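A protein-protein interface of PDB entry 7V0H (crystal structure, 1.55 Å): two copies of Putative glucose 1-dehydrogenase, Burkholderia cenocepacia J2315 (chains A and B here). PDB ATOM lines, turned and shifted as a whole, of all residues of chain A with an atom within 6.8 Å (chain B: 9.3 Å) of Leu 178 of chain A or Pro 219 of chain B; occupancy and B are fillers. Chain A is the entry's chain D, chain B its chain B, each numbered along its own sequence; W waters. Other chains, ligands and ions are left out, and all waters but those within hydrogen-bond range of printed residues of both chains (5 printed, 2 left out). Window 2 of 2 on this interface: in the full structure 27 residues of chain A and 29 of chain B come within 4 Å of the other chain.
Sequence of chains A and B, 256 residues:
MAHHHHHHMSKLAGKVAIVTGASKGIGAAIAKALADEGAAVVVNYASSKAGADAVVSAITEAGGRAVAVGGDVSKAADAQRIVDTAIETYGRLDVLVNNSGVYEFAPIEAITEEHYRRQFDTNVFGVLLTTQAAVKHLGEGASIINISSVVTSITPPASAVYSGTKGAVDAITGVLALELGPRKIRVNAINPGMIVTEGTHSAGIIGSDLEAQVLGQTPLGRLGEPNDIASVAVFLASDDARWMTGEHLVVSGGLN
Of chain B, only Pro 219 (3.5 Å) comes within 4 Å of Leu 178 of chain A. No residue of chain B comes within 4 Å of Ala 177 of chain A. Of chain B, only Pro 219 and Leu 220 come within 4 Å of Gly 181 of chain A. Printed residues of chain A within 4 Å of Leu 223 of chain B: Trp 243. Of the printed residues of chain A, Ser 252 of chain B touches Trp 243 (3.3 Å). Of the printed residues of chain A, Gly 253 of chain B touches Trp 243 and Thr 245. Of the printed residues of chain A, Gly 254 of chain B touches Thr 245 (3.4 Å). Leu 215 of chain B touches none of the printed residues of chain A. The nearest printed residue of chain A that does not touch Pro 219 of chain B is Pro 182 of chain A (4.003 Å).
Pro 219 of chain B touches Leu 178 of chain A (CG to CD2, 3.5 Å). CD2 of Leu 220 of chain B touches O of Gly 181 of chain A, at 3.96 Å. CE of Lys 184 of chain A touches O of Leu 220 of chain B (3.7 Å). CG2 of Thr 218 of chain B touches CH2 of Trp 243 of chain A, 3.95 Å away. Leu 220 of chain B touches Trp 243 of chain A. CH2 of Trp 243 of chain A touches O of Arg 222 of chain B, at 3.1 Å. Leu 223 of chain B touches Trp 243 of chain A. Thr 245 of chain A touches Leu 220 of chain B. Gly 253 of chain B touches Thr 245 of chain A (O to CG2, 3.7 Å). Thr 245 of chain A touches Gly 254 of chain B.
Hydrophobic or aromatic side chains of chain A within 4 Å of the printed part of chain B: Leu 178 and Trp 243. Hydrophobic or aromatic side chains of chain B that line the printed part of chain A: Pro 219 and Leu 220.
No position is printed for both chains.
O of Val 214 of chain B is in hydrogen-bond range of OG1 of Thr 218 of chain B. N of Leu 220 of chain B is in hydrogen-bond range of O of Gly 253 of chain B (3.0 Å). N of Gly 254 of chain B lies close to OG of Ser 252 of chain B (3.4 Å). O of Leu 255 of chain B is in hydrogen-bond range of OG of Ser 252 of chain B. N of Val 187 of chain A lies within hydrogen-bond range of OG1 of Thr 245 of chain A, at 3.0 Å.
Water W1 bridges O of Gly 246 of chain A (2.7 Å) and ND2 of Asn 256 of chain B (3.2 Å). Water W3 bridges O of Gly 254 of chain B and O of Thr 245 of chain A. Water W2 lies within hydrogen-bond range of O of Gly 221 of chain B (2.8 Å) and NZ of Lys 184 of chain A (3.1 Å). Water W4 bridges O of Thr 245 of chain A and ND2 of Asn 256 of chain B. Water W5 lies within hydrogen-bond range of the side-chain amino group of Lys 184 of chain A, the backbone carbonyl oxygen of Gly 181 of chain A and the backbone carbonyl oxygen of Pro 219 of chain B.
O of Trp 243 of chain A sits at hydrogen-bond distance from N of Ser 252 of chain B (3.3 Å). N of Gly 253 of chain B lies within hydrogen-bond range of O of Trp 243 of chain A, at 2.9 Å. O of Pro 219 of chain B sits close to O of Gly 181 of chain A, at 3.3 Å.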
ATOM      1  N   THR A 173      25.854 -18.954  18.821  1.00  0.00           N
ATOM      2  CA  THR A 173      24.970 -19.297  19.930  1.00  0.00           C
ATOM      3  C   THR A 173      24.433 -20.715  19.783  1.00  0.00           C
ATOM      4  O   THR A 173      24.481 -21.518  20.729  1.00  0.00           O
ATOM      5  CB  THR A 173      23.825 -18.273  19.992  1.00  0.00           C
ATOM      6  OG1 THR A 173      24.374 -16.974  20.211  1.00  0.00           O
ATOM      7  CG2 THR A 173      22.877 -18.589  21.150  1.00  0.00           C
ATOM      8  N   GLY A 174      23.946 -21.058  18.588  1.00  0.00           N
ATOM      9  CA  GLY A 174      23.432 -22.400  18.387  1.00  0.00           C
ATOM     10  C   GLY A 174      24.528 -23.447  18.486  1.00  0.00           C
ATOM     11  O   GLY A 174      24.325 -24.517  19.084  1.00  0.00           O
ATOM     12  N   VAL A 175      25.713 -23.162  17.911  1.00  0.00           N
ATOM     13  CA  VAL A 175      26.816 -24.126  17.995  1.00  0.00           C
ATOM     14  C   VAL A 175      27.170 -24.413  19.443  1.00  0.00           C
ATOM     15  O   VAL A 175      27.317 -25.578  19.837  1.00  0.00           O
ATOM     16  CB  VAL A 175      28.062 -23.630  17.241  1.00  0.00           C
ATOM     17  CG1 VAL A 175      29.285 -24.480  17.612  1.00  0.00           C
ATOM     18  CG2 VAL A 175      27.845 -23.655  15.719  1.00  0.00           C
ATOM     19  N   LEU A 176      27.375 -23.350  20.232  1.00  0.00           N
ATOM     20  CA  LEU A 176      27.882 -23.540  21.590  1.00  0.00           C
ATOM     21  C   LEU A 176      26.822 -24.153  22.485  1.00  0.00           C
ATOM     22  O   LEU A 176      27.162 -24.883  23.416  1.00  0.00           O
ATOM     23  CB  LEU A 176      28.409 -22.216  22.160  1.00  0.00           C
ATOM     24  CG  LEU A 176      29.643 -21.688  21.421  1.00  0.00           C
ATOM     25  CD1 LEU A 176      30.131 -20.404  22.085  1.00  0.00           C
ATOM     26  CD2 LEU A 176      30.757 -22.725  21.415  1.00  0.00           C
ATOM     27  N   ALA A 177      25.540 -23.913  22.196  1.00  0.00           N
ATOM     28  CA  ALA A 177      24.490 -24.605  22.933  1.00  0.00           C
ATOM     29  C   ALA A 177      24.614 -26.116  22.763  1.00  0.00           C
ATOM     30  O   ALA A 177      24.488 -26.872  23.736  1.00  0.00           O
ATOM     31  CB  ALA A 177      23.116 -24.104  22.475  1.00  0.00           C
ATOM     32  N   LEU A 178      24.884 -26.584  21.540  1.00  0.00           N
ATOM     33  CA  LEU A 178      25.076 -28.022  21.345  1.00  0.00           C
ATOM     34  C   LEU A 178      26.416 -28.483  21.906  1.00  0.00           C
ATOM     35  O   LEU A 178      26.516 -29.564  22.511  1.00  0.00           O
ATOM     36  CB  LEU A 178      24.999 -28.376  19.859  1.00  0.00           C
ATOM     37  CG  LEU A 178      23.649 -28.116  19.184  1.00  0.00           C
ATOM     38  CD1 LEU A 178      23.651 -28.736  17.791  1.00  0.00           C
ATOM     39  CD2 LEU A 178      22.462 -28.601  20.027  1.00  0.00           C
ATOM     40  N   GLU A 179      27.465 -27.699  21.678  1.00  0.00           N
ATOM     41  CA  GLU A 179      28.806 -28.130  22.077  1.00  0.00           C
ATOM     42  C   GLU A 179      28.937 -28.234  23.590  1.00  0.00           C
ATOM     43  O   GLU A 179      29.638 -29.127  24.091  1.00  0.00           O
ATOM     44  CB  GLU A 179      29.830 -27.146  21.529  1.00  0.00           C
ATOM     45  CG  GLU A 179      31.276 -27.577  21.679  1.00  0.00           C
ATOM     46  CD  GLU A 179      32.220 -26.568  21.056  1.00  0.00           C
ATOM     47  OE1 GLU A 179      31.955 -26.149  19.907  1.00  0.00           O
ATOM     48  OE2 GLU A 179      33.220 -26.193  21.701  1.00  0.00           O
ATOM     49  N   LEU A 180      28.298 -27.317  24.332  1.00  0.00           N
ATOM     50  CA  LEU A 180      28.414 -27.248  25.791  1.00  0.00           C
ATOM     51  C   LEU A 180      27.231 -27.893  26.487  1.00  0.00           C
ATOM     52  O   LEU A 180      27.219 -27.969  27.721  1.00  0.00           O
ATOM     53  CB  LEU A 180      28.537 -25.782  26.243  1.00  0.00           C
ATOM     54  CG  LEU A 180      29.739 -25.071  25.606  1.00  0.00           C
ATOM     55  CD1 LEU A 180      29.785 -23.634  26.105  1.00  0.00           C
ATOM     56  CD2 LEU A 180      31.066 -25.785  25.936  1.00  0.00           C
ATOM     57  N   GLY A 181      26.264 -28.398  25.723  1.00  0.00           N
ATOM     58  CA  GLY A 181      25.159 -29.175  26.263  1.00  0.00           C
ATOM     59  C   GLY A 181      25.567 -30.277  27.225  1.00  0.00           C
ATOM     60  O   GLY A 181      24.987 -30.443  28.302  1.00  0.00           O
ATOM     61  N   PRO A 182      26.546 -31.083  26.831  1.00  0.00           N
ATOM     62  CA  PRO A 182      26.955 -32.188  27.706  1.00  0.00           C
ATOM     63  C   PRO A 182      27.451 -31.727  29.071  1.00  0.00           C
ATOM     64  O   PRO A 182      27.463 -32.538  30.016  1.00  0.00           O
ATOM     65  CB  PRO A 182      28.075 -32.860  26.905  1.00  0.00           C
ATOM     66  CG  PRO A 182      27.717 -32.555  25.472  1.00  0.00           C
ATOM     67  CD  PRO A 182      27.228 -31.142  25.524  1.00  0.00           C
ATOM     68  N   ARG A 183      27.895 -30.481  29.185  1.00  0.00           N
ATOM     69  CA  ARG A 183      28.326 -29.906  30.453  1.00  0.00           C
ATOM     70  C   ARG A 183      27.192 -29.159  31.144  1.00  0.00           C
ATOM     71  O   ARG A 183      27.386 -28.625  32.248  1.00  0.00           O
ATOM     72  CB  ARG A 183      29.523 -28.974  30.216  1.00  0.00           C
ATOM     73  CG  ARG A 183      30.782 -29.772  29.851  1.00  0.00           C
ATOM     74  CD  ARG A 183      31.893 -28.845  29.351  1.00  0.00           C
ATOM     75  NE  ARG A 183      32.368 -27.963  30.409  1.00  0.00           N
ATOM     76  CZ  ARG A 183      33.275 -27.019  30.219  1.00  0.00           C
ATOM     77  NH1 ARG A 183      33.816 -26.816  29.029  1.00  0.00           N
ATOM     78  NH2 ARG A 183      33.645 -26.255  31.250  1.00  0.00           N
ATOM     79  N   LYS A 184      26.009 -29.163  30.530  1.00  0.00           N
ATOM     80  CA  LYS A 184      24.816 -28.475  31.030  1.00  0.00           C
ATOM     81  C   LYS A 184      25.077 -26.989  31.269  1.00  0.00           C
ATOM     82  O   LYS A 184      24.528 -26.379  32.190  1.00  0.00           O
ATOM     83  CB  LYS A 184      24.252 -29.190  32.263  1.00  0.00           C
ATOM     84  CG  LYS A 184      23.783 -30.620  31.907  1.00  0.00           C
ATOM     85  CD  LYS A 184      23.316 -31.407  33.097  1.00  0.00           C
ATOM     86  CE  LYS A 184      22.783 -32.783  32.669  1.00  0.00           C
ATOM     87  NZ  LYS A 184      23.786 -33.523  31.845  1.00  0.00           N
ATOM     88  N   ILE A 185      25.910 -26.407  30.402  1.00  0.00           N
ATOM     89  CA  ILE A 185      26.079 -24.965  30.296  1.00  0.00           C
ATOM     90  C   ILE A 185      25.099 -24.482  29.232  1.00  0.00           C
ATOM     91  O   ILE A 185      25.125 -24.981  28.104  1.00  0.00           O
ATOM     92  CB  ILE A 185      27.513 -24.630  29.882  1.00  0.00           C
ATOM     93  CG1 ILE A 185      28.490 -25.139  30.943  1.00  0.00           C
ATOM     94  CG2 ILE A 185      27.656 -23.138  29.636  1.00  0.00           C
ATOM     95  CD1 ILE A 185      29.961 -25.070  30.481  1.00  0.00           C
ATOM     96  N   VAL A 187      23.484 -21.752  26.558  1.00  0.00           N
ATOM     97  CA  VAL A 187      23.949 -20.656  25.702  1.00  0.00           C
ATOM     98  C   VAL A 187      22.729 -20.148  24.943  1.00  0.00           C
ATOM     99  O   VAL A 187      22.084 -20.911  24.222  1.00  0.00           O
ATOM    100  CB  VAL A 187      25.056 -21.102  24.713  1.00  0.00           C
ATOM    101  CG1 VAL A 187      25.666 -19.908  23.997  1.00  0.00           C
ATOM    102  CG2 VAL A 187      26.174 -21.855  25.434  1.00  0.00           C
ATOM    103  N   TRP A 243      15.577 -24.815  31.140  1.00  0.00           N
ATOM    104  CA  TRP A 243      15.268 -25.745  30.064  1.00  0.00           C
ATOM    105  C   TRP A 243      15.318 -25.066  28.695  1.00  0.00           C
ATOM    106  O   TRP A 243      14.804 -25.608  27.707  1.00  0.00           O
ATOM    107  CB  TRP A 243      13.917 -26.425  30.340  1.00  0.00           C
ATOM    108  CG  TRP A 243      13.764 -27.753  29.675  1.00  0.00           C
ATOM    109  CD1 TRP A 243      12.697 -28.184  28.926  1.00  0.00           C
ATOM    110  CD2 TRP A 243      14.690 -28.842  29.710  1.00  0.00           C
ATOM    111  NE1 TRP A 243      12.920 -29.462  28.476  1.00  0.00           N
ATOM    112  CE2 TRP A 243      14.133 -29.890  28.949  1.00  0.00           C
ATOM    113  CE3 TRP A 243      15.938 -29.031  30.306  1.00  0.00           C
ATOM    114  CZ2 TRP A 243      14.785 -31.105  28.758  1.00  0.00           C
ATOM    115  CZ3 TRP A 243      16.586 -30.249  30.114  1.00  0.00           C
ATOM    116  CH2 TRP A 243      16.014 -31.256  29.344  1.00  0.00           C
ATOM    117  N   THR A 245      18.045 -23.631  25.882  1.00  0.00           N
ATOM    118  CA  THR A 245      19.389 -23.391  25.376  1.00  0.00           C
ATOM    119  C   THR A 245      19.349 -23.386  23.854  1.00  0.00           C
ATOM    120  O   THR A 245      18.542 -24.083  23.234  1.00  0.00           O
ATOM    121  CB  THR A 245      20.394 -24.422  25.952  1.00  0.00           C
ATOM    122  OG1 THR A 245      21.731 -24.012  25.637  1.00  0.00           O
ATOM    123  CG2 THR A 245      20.198 -25.840  25.379  1.00  0.00           C
ATOM    124  N   GLY A 246      20.189 -22.540  23.257  1.00  0.00           N
ATOM    125  CA  GLY A 246      20.166 -22.406  21.805  1.00  0.00           C
ATOM    126  C   GLY A 246      19.060 -21.527  21.282  1.00  0.00           C
ATOM    127  O   GLY A 246      18.799 -21.553  20.066  1.00  0.00           O
ATOM    128  N   GLN B 213      13.936 -41.275  20.811  1.00  0.00           N
ATOM    129  CA  GLN B 213      14.546 -40.400  19.816  1.00  0.00           C
ATOM    130  C   GLN B 213      14.746 -39.002  20.369  1.00  0.00           C
ATOM    131  O   GLN B 213      15.794 -38.384  20.156  1.00  0.00           O
ATOM    132  CB  GLN B 213      13.676 -40.338  18.557  1.00  0.00           C
ATOM    133  CG  GLN B 213      13.502 -41.649  17.827  1.00  0.00           C
ATOM    134  CD  GLN B 213      14.748 -42.081  17.062  1.00  0.00           C
ATOM    135  OE1 GLN B 213      15.355 -41.296  16.323  1.00  0.00           O
ATOM    136  NE2 GLN B 213      15.138 -43.341  17.237  1.00  0.00           N
ATOM    137  N   VAL B 214      13.750 -38.486  21.085  1.00  0.00           N
ATOM    138  CA  VAL B 214      13.857 -37.135  21.619  1.00  0.00           C
ATOM    139  C   VAL B 214      14.966 -37.066  22.655  1.00  0.00           C
ATOM    140  O   VAL B 214      15.820 -36.168  22.624  1.00  0.00           O
ATOM    141  CB  VAL B 214      12.500 -36.694  22.204  1.00  0.00           C
ATOM    142  CG1 VAL B 214      12.681 -35.495  23.103  1.00  0.00           C
ATOM    143  CG2 VAL B 214      11.533 -36.378  21.073  1.00  0.00           C
ATOM    144  N   LEU B 215      14.984 -38.022  23.579  1.00  0.00           N
ATOM    145  CA  LEU B 215      16.029 -38.022  24.592  1.00  0.00           C
ATOM    146  C   LEU B 215      17.415 -38.047  23.951  1.00  0.00           C
ATOM    147  O   LEU B 215      18.299 -37.281  24.340  1.00  0.00           O
ATOM    148  CB  LEU B 215      15.850 -39.202  25.544  1.00  0.00           C
ATOM    149  CG  LEU B 215      16.804 -39.176  26.740  1.00  0.00           C
ATOM    150  CD1 LEU B 215      16.697 -37.857  27.500  1.00  0.00           C
ATOM    151  CD2 LEU B 215      16.489 -40.330  27.653  1.00  0.00           C
ATOM    152  N   GLY B 216      17.608 -38.898  22.938  1.00  0.00           N
ATOM    153  CA  GLY B 216      18.892 -39.047  22.285  1.00  0.00           C
ATOM    154  C   GLY B 216      19.352 -37.827  21.521  1.00  0.00           C
ATOM    155  O   GLY B 216      20.521 -37.771  21.125  1.00  0.00           O
ATOM    156  N   GLN B 217      18.462 -36.850  21.323  1.00  0.00           N
ATOM    157  CA  GLN B 217      18.790 -35.610  20.627  1.00  0.00           C
ATOM    158  C   GLN B 217      18.601 -34.376  21.498  1.00  0.00           C
ATOM    159  O   GLN B 217      18.600 -33.251  20.974  1.00  0.00           O
ATOM    160  CB  GLN B 217      17.954 -35.489  19.341  1.00  0.00           C
ATOM    161  CG  GLN B 217      18.329 -36.544  18.299  1.00  0.00           C
ATOM    162  CD  GLN B 217      19.735 -36.335  17.747  1.00  0.00           C
ATOM    163  OE1 GLN B 217      20.225 -35.198  17.675  1.00  0.00           O
ATOM    164  NE2 GLN B 217      20.403 -37.433  17.354  1.00  0.00           N
ATOM    165  N   THR B 218      18.436 -34.540  22.816  1.00  0.00           N
ATOM    166  CA  THR B 218      18.227 -33.388  23.685  1.00  0.00           C
ATOM    167  C   THR B 218      19.555 -32.952  24.288  1.00  0.00           C
ATOM    168  O   THR B 218      20.162 -33.717  25.058  1.00  0.00           O
ATOM    169  CB  THR B 218      17.215 -33.722  24.784  1.00  0.00           C
ATOM    170  OG1 THR B 218      15.937 -34.010  24.183  1.00  0.00           O
ATOM    171  CG2 THR B 218      17.070 -32.566  25.766  1.00  0.00           C
ATOM    172  N   PRO B 219      20.045 -31.753  23.964  1.00  0.00           N
ATOM    173  CA  PRO B 219      21.370 -31.337  24.446  1.00  0.00           C
ATOM    174  C   PRO B 219      21.534 -31.372  25.960  1.00  0.00           C
ATOM    175  O   PRO B 219      22.617 -31.743  26.442  1.00  0.00           O
ATOM    176  CB  PRO B 219      21.486 -29.909  23.893  1.00  0.00           C
ATOM    177  CG  PRO B 219      20.682 -29.960  22.652  1.00  0.00           C
ATOM    178  CD  PRO B 219      19.500 -30.820  22.963  1.00  0.00           C
ATOM    179  N   LEU B 220      20.491 -31.015  26.724  1.00  0.00           N
ATOM    180  CA  LEU B 220      20.636 -30.954  28.177  1.00  0.00           C
ATOM    181  C   LEU B 220      20.267 -32.268  28.853  1.00  0.00           C
ATOM    182  O   LEU B 220      20.204 -32.321  30.085  1.00  0.00           O
ATOM    183  CB  LEU B 220      19.814 -29.787  28.739  1.00  0.00           C
ATOM    184  CG  LEU B 220      20.373 -28.408  28.310  1.00  0.00           C
ATOM    185  CD1 LEU B 220      19.471 -27.309  28.812  1.00  0.00           C
ATOM    186  CD2 LEU B 220      21.783 -28.183  28.857  1.00  0.00           C
ATOM    187  N   GLY B 221      20.058 -33.332  28.083  1.00  0.00           N
ATOM    188  CA  GLY B 221      20.293 -34.660  28.627  1.00  0.00           C
ATOM    189  C   GLY B 221      19.219 -35.262  29.515  1.00  0.00           C
ATOM    190  O   GLY B 221      19.535 -36.141  30.330  1.00  0.00           O
ATOM    191  N   ARG B 222      17.958 -34.869  29.350  1.00  0.00           N
ATOM    192  CA  ARG B 222      16.850 -35.441  30.112  1.00  0.00           C
ATOM    193  C   ARG B 222      15.555 -35.044  29.421  1.00  0.00           C
ATOM    194  O   ARG B 222      15.549 -34.197  28.519  1.00  0.00           O
ATOM    195  CB  ARG B 222      16.868 -34.973  31.570  1.00  0.00           C
ATOM    196  CG  ARG B 222      16.691 -33.451  31.721  1.00  0.00           C
ATOM    197  CD  ARG B 222      16.468 -33.096  33.187  1.00  0.00           C
ATOM    198  NE  ARG B 222      16.423 -31.660  33.442  1.00  0.00           N
ATOM    199  CZ  ARG B 222      15.318 -30.924  33.373  1.00  0.00           C
ATOM    200  NH1 ARG B 222      14.162 -31.444  32.977  1.00  0.00           N
ATOM    201  NH2 ARG B 222      15.371 -29.632  33.707  1.00  0.00           N
ATOM    202  N   LEU B 223      14.452 -35.673  29.839  1.00  0.00           N
ATOM    203  CA  LEU B 223      13.142 -35.181  29.441  1.00  0.00           C
ATOM    204  C   LEU B 223      12.774 -33.956  30.268  1.00  0.00           C
ATOM    205  O   LEU B 223      13.259 -33.764  31.390  1.00  0.00           O
ATOM    206  CB  LEU B 223      12.075 -36.261  29.623  1.00  0.00           C
ATOM    207  CG  LEU B 223      12.321 -37.540  28.824  1.00  0.00           C
ATOM    208  CD1 LEU B 223      11.279 -38.567  29.196  1.00  0.00           C
ATOM    209  CD2 LEU B 223      12.297 -37.249  27.320  1.00  0.00           C
ATOM    210  N   VAL B 250      11.176 -21.828  22.486  1.00  0.00           N
ATOM    211  CA  VAL B 250      11.335 -23.280  22.510  1.00  0.00           C
ATOM    212  C   VAL B 250      11.940 -23.660  23.847  1.00  0.00           C
ATOM    213  O   VAL B 250      13.052 -23.232  24.176  1.00  0.00           O
ATOM    214  CB  VAL B 250      12.209 -23.770  21.354  1.00  0.00           C
ATOM    215  CG1 VAL B 250      12.490 -25.280  21.488  1.00  0.00           C
ATOM    216  CG2 VAL B 250      11.544 -23.443  20.025  1.00  0.00           C
ATOM    217  N   SER B 252      12.846 -26.876  25.439  1.00  0.00           N
ATOM    218  CA  SER B 252      12.976 -28.280  25.086  1.00  0.00           C
ATOM    219  C   SER B 252      14.326 -28.830  25.491  1.00  0.00           C
ATOM    220  O   SER B 252      14.673 -29.936  25.049  1.00  0.00           O
ATOM    221  CB  SER B 252      12.815 -28.467  23.597  1.00  0.00           C
ATOM    222  OG  SER B 252      13.934 -27.818  22.983  1.00  0.00           O
ATOM    223  N   GLY B 253      15.088 -28.103  26.306  1.00  0.00           N
ATOM    224  CA  GLY B 253      16.418 -28.573  26.641  1.00  0.00           C
ATOM    225  C   GLY B 253      17.382 -28.481  25.483  1.00  0.00           C
ATOM    226  O   GLY B 253      18.425 -29.140  25.495  1.00  0.00           O
ATOM    227  N   GLY B 254      17.036 -27.694  24.465  1.00  0.00           N
ATOM    228  CA  GLY B 254      17.938 -27.445  23.359  1.00  0.00           C
ATOM    229  C   GLY B 254      17.604 -28.148  22.069  1.00  0.00           C
ATOM    230  O   GLY B 254      18.360 -27.996  21.096  1.00  0.00           O
ATOM    231  N   LEU B 255      16.515 -28.916  22.021  1.00  0.00           N
ATOM    232  CA  LEU B 255      16.116 -29.608  20.806  1.00  0.00           C
ATOM    233  C   LEU B 255      15.282 -28.685  19.927  1.00  0.00           C
ATOM    234  O   LEU B 255      14.272 -28.156  20.379  1.00  0.00           O
ATOM    235  CB  LEU B 255      15.327 -30.867  21.168  1.00  0.00           C
ATOM    236  CG  LEU B 255      14.769 -31.672  19.999  1.00  0.00           C
ATOM    237  CD1 LEU B 255      15.886 -32.164  19.082  1.00  0.00           C
ATOM    238  CD2 LEU B 255      13.953 -32.831  20.542  1.00  0.00           C
ATOM    239  N   ASN B 256      15.732 -28.473  18.686  1.00  0.00           N
ATOM    240  CA  ASN B 256      14.958 -27.668  17.744  1.00  0.00           C
ATOM    241  C   ASN B 256      15.287 -28.026  16.293  1.00  0.00           C
ATOM    242  O   ASN B 256      16.098 -28.902  16.004  1.00  0.00           O
ATOM    243  CB  ASN B 256      15.167 -26.162  18.012  1.00  0.00           C
ATOM    244  CG  ASN B 256      16.593 -25.711  17.754  1.00  0.00           C
ATOM    245  OD1 ASN B 256      17.080 -25.781  16.619  1.00  0.00           O
ATOM    246  ND2 ASN B 256      17.265 -25.223  18.800  1.00  0.00           N
ATOM    247  OXT ASN B 256      14.689 -27.473  15.360  1.00  0.00           O
HETATM  248  O   HOH W   1      19.714 -23.253  18.158  1.00  0.00           O
HETATM  249  O   HOH W   2      21.879 -36.002  31.770  1.00  0.00           O
HETATM  250  O   HOH W   3      20.179 -25.983  21.417  1.00  0.00           O
HETATM  251  O   HOH W   4      16.362 -24.426  21.566  1.00  0.00           O
HETATM  252  O   HOH W   5      23.719 -32.985  29.122  1.00  0.00           O
